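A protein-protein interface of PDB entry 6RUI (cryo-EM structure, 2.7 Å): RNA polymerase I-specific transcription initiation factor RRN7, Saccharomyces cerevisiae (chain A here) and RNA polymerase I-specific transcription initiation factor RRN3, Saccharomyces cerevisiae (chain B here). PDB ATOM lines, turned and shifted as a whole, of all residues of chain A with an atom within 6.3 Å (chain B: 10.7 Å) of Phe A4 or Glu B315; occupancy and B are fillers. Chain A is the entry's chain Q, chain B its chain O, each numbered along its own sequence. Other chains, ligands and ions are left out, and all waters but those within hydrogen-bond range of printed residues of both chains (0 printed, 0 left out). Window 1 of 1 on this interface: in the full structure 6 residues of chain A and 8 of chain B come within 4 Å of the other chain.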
ATOM      1  N   THR A   3      21.334  -0.325 -27.505  1.00  0.00           N
ATOM      2  CA  THR A   3      20.705   0.202 -28.701  1.00  0.00           C
ATOM      3  C   THR A   3      19.184   0.152 -28.556  1.00  0.00           C
ATOM      4  O   THR A   3      18.448   0.445 -29.497  1.00  0.00           O
ATOM      5  CB  THR A   3      21.149  -0.579 -29.948  1.00  0.00           C
ATOM      6  OG1 THR A   3      20.705  -1.937 -29.850  1.00  0.00           O
ATOM      7  CG2 THR A   3      22.665  -0.566 -30.054  1.00  0.00           C
ATOM      8  N   PHE A   4      18.725  -0.206 -27.360  1.00  0.00           N
ATOM      9  CA  PHE A   4      17.305  -0.276 -27.042  1.00  0.00           C
ATOM     10  C   PHE A   4      16.782   1.117 -26.726  1.00  0.00           C
ATOM     11  O   PHE A   4      17.478   1.922 -26.101  1.00  0.00           O
ATOM     12  CB  PHE A   4      17.055  -1.194 -25.845  1.00  0.00           C
ATOM     13  CG  PHE A   4      17.312  -2.647 -26.113  1.00  0.00           C
ATOM     14  CD1 PHE A   4      16.311  -3.461 -26.588  1.00  0.00           C
ATOM     15  CD2 PHE A   4      18.565  -3.196 -25.891  1.00  0.00           C
ATOM     16  CE1 PHE A   4      16.546  -4.793 -26.821  1.00  0.00           C
ATOM     17  CE2 PHE A   4      18.802  -4.527 -26.136  1.00  0.00           C
ATOM     18  CZ  PHE A   4      17.790  -5.323 -26.602  1.00  0.00           C
ATOM     19  N   ILE A   5      15.549   1.393 -27.151  1.00  0.00           N
ATOM     20  CA  ILE A   5      14.917   2.685 -26.926  1.00  0.00           C
ATOM     21  C   ILE A   5      13.711   2.489 -26.017  1.00  0.00           C
ATOM     22  O   ILE A   5      13.083   1.427 -26.014  1.00  0.00           O
ATOM     23  CB  ILE A   5      14.513   3.377 -28.250  1.00  0.00           C
ATOM     24  CG1 ILE A   5      13.467   2.565 -29.017  1.00  0.00           C
ATOM     25  CG2 ILE A   5      15.738   3.610 -29.129  1.00  0.00           C
ATOM     26  CD1 ILE A   5      12.882   3.304 -30.207  1.00  0.00           C
ATOM     27  N   ARG A   6      13.389   3.533 -25.248  1.00  0.00           N
ATOM     28  CA  ARG A   6      12.365   3.477 -24.208  1.00  0.00           C
ATOM     29  C   ARG A   6      10.956   3.623 -24.773  1.00  0.00           C
ATOM     30  O   ARG A   6      10.711   3.541 -25.979  1.00  0.00           O
ATOM     31  CB  ARG A   6      12.593   4.555 -23.155  1.00  0.00           C
ATOM     32  CG  ARG A   6      13.748   4.326 -22.234  1.00  0.00           C
ATOM     33  CD  ARG A   6      13.481   3.194 -21.257  1.00  0.00           C
ATOM     34  NE  ARG A   6      12.337   3.456 -20.388  1.00  0.00           N
ATOM     35  CZ  ARG A   6      11.766   2.545 -19.602  1.00  0.00           C
ATOM     36  NH1 ARG A   6      12.252   1.308 -19.558  1.00  0.00           N
ATOM     37  NH2 ARG A   6      10.728   2.866 -18.848  1.00  0.00           N
ATOM     38  N   ARG A  18      12.042  -1.383 -21.357  1.00  0.00           N
ATOM     39  CA  ARG A  18      11.965  -1.105 -22.780  1.00  0.00           C
ATOM     40  C   ARG A  18      12.218  -2.383 -23.584  1.00  0.00           C
ATOM     41  O   ARG A  18      12.926  -3.298 -23.150  1.00  0.00           O
ATOM     42  CB  ARG A  18      12.964  -0.014 -23.157  1.00  0.00           C
ATOM     43  CG  ARG A  18      14.405  -0.445 -23.410  1.00  0.00           C
ATOM     44  CD  ARG A  18      15.162  -0.799 -22.139  1.00  0.00           C
ATOM     45  NE  ARG A  18      15.259   0.332 -21.226  1.00  0.00           N
ATOM     46  CZ  ARG A  18      15.321   0.228 -19.905  1.00  0.00           C
ATOM     47  NH1 ARG A  18      15.415   1.306 -19.155  1.00  0.00           N
ATOM     48  NH2 ARG A  18      15.305  -0.971 -19.328  1.00  0.00           N
ATOM     49  N   LEU A  19      11.619  -2.441 -24.771  1.00  0.00           N
ATOM     50  CA  LEU A  19      11.477  -3.683 -25.518  1.00  0.00           C
ATOM     51  C   LEU A  19      12.338  -3.630 -26.772  1.00  0.00           C
ATOM     52  O   LEU A  19      13.171  -2.740 -26.951  1.00  0.00           O
ATOM     53  CB  LEU A  19      10.018  -3.950 -25.896  1.00  0.00           C
ATOM     54  CG  LEU A  19       8.983  -4.268 -24.819  1.00  0.00           C
ATOM     55  CD1 LEU A  19       8.390  -2.983 -24.279  1.00  0.00           C
ATOM     56  CD2 LEU A  19       7.900  -5.191 -25.344  1.00  0.00           C
ATOM     57  N   TRP A  20      12.130  -4.601 -27.652  1.00  0.00           N
ATOM     58  CA  TRP A  20      12.898  -4.706 -28.884  1.00  0.00           C
ATOM     59  C   TRP A  20      11.945  -4.820 -30.060  1.00  0.00           C
ATOM     60  O   TRP A  20      11.307  -5.860 -30.244  1.00  0.00           O
ATOM     61  CB  TRP A  20      13.840  -5.896 -28.820  1.00  0.00           C
ATOM     62  CG  TRP A  20      14.687  -6.006 -30.006  1.00  0.00           C
ATOM     63  CD1 TRP A  20      15.404  -5.012 -30.582  1.00  0.00           C
ATOM     64  CD2 TRP A  20      15.008  -7.200 -30.714  1.00  0.00           C
ATOM     65  NE1 TRP A  20      16.111  -5.496 -31.651  1.00  0.00           N
ATOM     66  CE2 TRP A  20      15.890  -6.844 -31.748  1.00  0.00           C
ATOM     67  CE3 TRP A  20      14.618  -8.536 -30.590  1.00  0.00           C
ATOM     68  CZ2 TRP A  20      16.389  -7.774 -32.655  1.00  0.00           C
ATOM     69  CZ3 TRP A  20      15.112  -9.454 -31.490  1.00  0.00           C
ATOM     70  CH2 TRP A  20      15.994  -9.072 -32.504  1.00  0.00           C
ATOM     71  N   ARG A  21      11.848  -3.756 -30.851  1.00  0.00           N
ATOM     72  CA  ARG A  21      10.960  -3.743 -32.004  1.00  0.00           C
ATOM     73  C   ARG A  21      11.633  -4.516 -33.126  1.00  0.00           C
ATOM     74  O   ARG A  21      12.861  -4.487 -33.254  1.00  0.00           O
ATOM     75  CB  ARG A  21      10.583  -2.319 -32.426  1.00  0.00           C
ATOM     76  CG  ARG A  21      11.516  -1.556 -33.355  1.00  0.00           C
ATOM     77  CD  ARG A  21      12.773  -1.053 -32.663  1.00  0.00           C
ATOM     78  NE  ARG A  21      13.582  -0.224 -33.556  1.00  0.00           N
ATOM     79  CZ  ARG A  21      14.452  -0.702 -34.442  1.00  0.00           C
ATOM     80  NH1 ARG A  21      14.631  -2.011 -34.565  1.00  0.00           N
ATOM     81  NH2 ARG A  21      15.140   0.127 -35.214  1.00  0.00           N
ATOM     82  N   GLN A  30      12.355  -9.356 -24.885  1.00  0.00           N
ATOM     83  CA  GLN A  30      13.760  -9.720 -24.875  1.00  0.00           C
ATOM     84  C   GLN A  30      13.983 -11.218 -24.984  1.00  0.00           C
ATOM     85  O   GLN A  30      15.117 -11.640 -25.210  1.00  0.00           O
ATOM     86  CB  GLN A  30      14.420  -9.195 -23.597  1.00  0.00           C
ATOM     87  CG  GLN A  30      14.398  -7.677 -23.470  1.00  0.00           C
ATOM     88  CD  GLN A  30      15.050  -7.199 -22.192  1.00  0.00           C
ATOM     89  OE1 GLN A  30      15.456  -8.001 -21.353  1.00  0.00           O
ATOM     90  NE2 GLN A  30      15.158  -5.887 -22.037  1.00  0.00           N
ATOM     91  N   GLU B 309      11.639   6.307 -11.439  1.00  0.00           N
ATOM     92  CA  GLU B 309      11.672   7.764 -11.440  1.00  0.00           C
ATOM     93  C   GLU B 309      10.870   8.368 -12.586  1.00  0.00           C
ATOM     94  O   GLU B 309      11.214   9.450 -13.082  1.00  0.00           O
ATOM     95  CB  GLU B 309      13.121   8.260 -11.467  1.00  0.00           C
ATOM     96  CG  GLU B 309      13.872   7.980 -10.166  1.00  0.00           C
ATOM     97  CD  GLU B 309      15.311   8.460 -10.172  1.00  0.00           C
ATOM     98  OE1 GLU B 309      15.800   8.896 -11.234  1.00  0.00           O
ATOM     99  OE2 GLU B 309      15.953   8.403  -9.104  1.00  0.00           O
ATOM    100  N   MET B 311      10.537   7.880 -15.910  1.00  0.00           N
ATOM    101  CA  MET B 311      11.159   7.206 -17.033  1.00  0.00           C
ATOM    102  C   MET B 311      12.491   6.650 -16.565  1.00  0.00           C
ATOM    103  O   MET B 311      12.861   6.762 -15.393  1.00  0.00           O
ATOM    104  CB  MET B 311      11.359   8.136 -18.237  1.00  0.00           C
ATOM    105  CG  MET B 311      12.318   9.288 -17.994  1.00  0.00           C
ATOM    106  SD  MET B 311      12.599  10.253 -19.496  1.00  0.00           S
ATOM    107  CE  MET B 311      11.001  11.029 -19.717  1.00  0.00           C
ATOM    108  N   ASP B 312      13.209   6.026 -17.490  1.00  0.00           N
ATOM    109  CA  ASP B 312      14.516   5.465 -17.193  1.00  0.00           C
ATOM    110  C   ASP B 312      15.619   6.091 -18.032  1.00  0.00           C
ATOM    111  O   ASP B 312      16.612   6.576 -17.478  1.00  0.00           O
ATOM    112  CB  ASP B 312      14.483   3.945 -17.402  1.00  0.00           C
ATOM    113  CG  ASP B 312      13.570   3.228 -16.415  1.00  0.00           C
ATOM    114  OD1 ASP B 312      13.394   3.730 -15.286  1.00  0.00           O
ATOM    115  OD2 ASP B 312      13.038   2.155 -16.763  1.00  0.00           O
ATOM    116  N   GLY B 313      15.465   6.115 -19.346  1.00  0.00           N
ATOM    117  CA  GLY B 313      16.515   6.493 -20.280  1.00  0.00           C
ATOM    118  C   GLY B 313      16.878   5.287 -21.130  1.00  0.00           C
ATOM    119  O   GLY B 313      16.913   4.151 -20.641  1.00  0.00           O
ATOM    120  N   THR B 314      17.127   5.529 -22.418  1.00  0.00           N
ATOM    121  CA  THR B 314      17.295   4.446 -23.384  1.00  0.00           C
ATOM    122  C   THR B 314      18.588   3.681 -23.132  1.00  0.00           C
ATOM    123  O   THR B 314      19.625   4.270 -22.815  1.00  0.00           O
ATOM    124  CB  THR B 314      17.287   5.001 -24.806  1.00  0.00           C
ATOM    125  OG1 THR B 314      18.407   5.878 -24.985  1.00  0.00           O
ATOM    126  CG2 THR B 314      15.999   5.772 -25.064  1.00  0.00           C
ATOM    127  N   GLU B 315      18.528   2.358 -23.290  1.00  0.00           N
ATOM    128  CA  GLU B 315      19.590   1.513 -22.762  1.00  0.00           C
ATOM    129  C   GLU B 315      20.286   0.685 -23.834  1.00  0.00           C
ATOM    130  O   GLU B 315      20.050   0.883 -25.031  1.00  0.00           O
ATOM    131  CB  GLU B 315      19.045   0.597 -21.668  1.00  0.00           C
ATOM    132  CG  GLU B 315      18.559   1.328 -20.436  1.00  0.00           C
ATOM    133  CD  GLU B 315      19.654   2.052 -19.681  1.00  0.00           C
ATOM    134  OE1 GLU B 315      20.813   1.584 -19.688  1.00  0.00           O
ATOM    135  OE2 GLU B 315      19.344   3.092 -19.060  1.00  0.00           O
ATOM    136  N   GLU B 316      21.128  -0.249 -23.404  1.00  0.00           N
ATOM    137  CA  GLU B 316      22.151  -0.850 -24.251  1.00  0.00           C
ATOM    138  C   GLU B 316      22.178  -2.351 -23.942  1.00  0.00           C
ATOM    139  O   GLU B 316      21.240  -2.904 -23.358  1.00  0.00           O
ATOM    140  CB  GLU B 316      23.459  -0.043 -24.046  1.00  0.00           C
ATOM    141  CG  GLU B 316      24.654  -0.270 -25.003  1.00  0.00           C
ATOM    142  CD  GLU B 316      24.327  -0.051 -26.469  1.00  0.00           C
ATOM    143  OE1 GLU B 316      23.455   0.785 -26.790  1.00  0.00           O
ATOM    144  OE2 GLU B 316      24.931  -0.750 -27.308  1.00  0.00           O
ATOM    145  N   TYR B 317      23.254  -3.028 -24.343  1.00  0.00           N
ATOM    146  CA  TYR B 317      23.404  -4.475 -24.440  1.00  0.00           C
ATOM    147  C   TYR B 317      23.644  -5.141 -23.095  1.00  0.00           C
ATOM    148  O   TYR B 317      23.227  -4.621 -22.052  1.00  0.00           O
ATOM    149  CB  TYR B 317      24.560  -4.825 -25.379  1.00  0.00           C
ATOM    150  CG  TYR B 317      24.298  -4.556 -26.842  1.00  0.00           C
ATOM    151  CD1 TYR B 317      23.009  -4.347 -27.317  1.00  0.00           C
ATOM    152  CD2 TYR B 317      25.345  -4.524 -27.750  1.00  0.00           C
ATOM    153  CE1 TYR B 317      22.774  -4.109 -28.646  1.00  0.00           C
ATOM    154  CE2 TYR B 317      25.121  -4.285 -29.084  1.00  0.00           C
ATOM    155  CZ  TYR B 317      23.835  -4.078 -29.528  1.00  0.00           C
ATOM    156  OH  TYR B 317      23.605  -3.840 -30.862  1.00  0.00           O
ATOM    157  N   ASN B 318      24.217  -6.350 -23.156  1.00  0.00           N
ATOM    158  CA  ASN B 318      24.610  -7.170 -22.004  1.00  0.00           C
ATOM    159  C   ASN B 318      23.370  -7.641 -21.243  1.00  0.00           C
ATOM    160  O   ASN B 318      23.242  -7.462 -20.033  1.00  0.00           O
ATOM    161  CB  ASN B 318      25.603  -6.439 -21.086  1.00  0.00           C
ATOM    162  CG  ASN B 318      26.377  -7.380 -20.185  1.00  0.00           C
ATOM    163  OD1 ASN B 318      26.217  -8.595 -20.250  1.00  0.00           O
ATOM    164  ND2 ASN B 318      27.221  -6.816 -19.333  1.00  0.00           N
ATOM    165  N   VAL B 319      22.440  -8.234 -21.997  1.00  0.00           N
ATOM    166  CA  VAL B 319      21.296  -8.935 -21.419  1.00  0.00           C
ATOM    167  C   VAL B 319      21.770 -10.127 -20.594  1.00  0.00           C
ATOM    168  O   VAL B 319      21.231 -10.405 -19.514  1.00  0.00           O
ATOM    169  CB  VAL B 319      20.332  -9.359 -22.547  1.00  0.00           C
ATOM    170  CG1 VAL B 319      19.165 -10.179 -22.012  1.00  0.00           C
ATOM    171  CG2 VAL B 319      19.832  -8.130 -23.309  1.00  0.00           C
ATOM    172  N   GLU B 320      22.819 -10.811 -21.081  1.00  0.00           N
ATOM    173  CA  GLU B 320      23.555 -11.920 -20.436  1.00  0.00           C
ATOM    174  C   GLU B 320      22.637 -13.000 -19.843  1.00  0.00           C
ATOM    175  O   GLU B 320      22.613 -13.259 -18.638  1.00  0.00           O
ATOM    176  CB  GLU B 320      24.605 -11.396 -19.424  1.00  0.00           C
ATOM    177  CG  GLU B 320      24.183 -10.524 -18.217  1.00  0.00           C
ATOM    178  CD  GLU B 320      25.359  -9.983 -17.428  1.00  0.00           C
ATOM    179  OE1 GLU B 320      26.515 -10.234 -17.829  1.00  0.00           O
ATOM    180  OE2 GLU B 320      25.127  -9.302 -16.406  1.00  0.00           O
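N of Thr A3 sits at hydrogen-bond distance from OE1 of Glu B316, 2.5 Å away.
The side-chain carboxylate (OD2) of Asp B312 is in salt-bridge range of the guanidinium group (NH1) of Arg A6, at 3.0 Å.
O of Glu B315 lies within hydrogen-bond range of N of Phe A4.
The side-chain carboxylate of Asp B312 is in salt-bridge range of the guanidinium group of Arg A18 (3.5 Å).
The backbone NH of Thr A3 lies within hydrogen-bond range of the backbone carbonyl oxygen of Glu B315 (3.0 Å).
Among the printed residues, merely in contact across the chains: Thr A3 with Tyr B317, Phe A4 with Thr B314, Arg A18 with Glu B315, Arg A6 with Thr B314, Arg A6 with Gly B313, Arg A18 with Gly B313, Phe A4 with Glu B316 and Ile A5 with Thr B314.
Of chain B, only Glu B315 (3.0 Å), Glu B316 (2.5 Å) and Tyr B317 (3.2 Å) come within 4 Å of Thr A3.
Of chain B, only Thr B314, Glu B315 and Glu B316 come within 4 Å of Phe A4.
Printed residues of chain A within 4 Å of Gly B313: Arg A6 and Arg A18.
Of the printed residues of chain A, Thr B314 touches Phe A4 (3.3 Å), Ile A5 (3.8 Å) and Arg A6 (3.4 Å).
Of chain A, only Thr A3, Phe A4 and Arg A18 come within 4 Å of Glu B315.
Of the printed residues of chain A, Glu B316 touches Thr A3 and Phe A4.
Of the printed residues of chain A, Tyr B317 touches Thr A3.
Glu B320 touches none of the printed residues of chain A.
The nearest residue of chain B that does not touch Phe A4 is Tyr B317 (4.4 Å).
The nearest residue of chain A that does not touch Glu B315 is Ile A5 (5.0 Å).
Printed residues of chain A that touch a printed residue of chain B: Thr A3, Phe A4, Ile A5, Arg A6 and Arg A18.
Hydrophobic or aromatic side chains of chain A within 4 Å of the printed part of chain B: Phe A4.
Hydrophobic or aromatic side chains of chain B within 4 Å of the printed part of chain A: Tyr B317.
Among the printed residues, 13 pairs touch across the chains.
Among the printed residues, Asp or Glu carboxylates within 4 Å of a Lys or Arg side-chain nitrogen of the other chain: Arg A6 with Asp B312 and Arg A18 with Asp B312.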
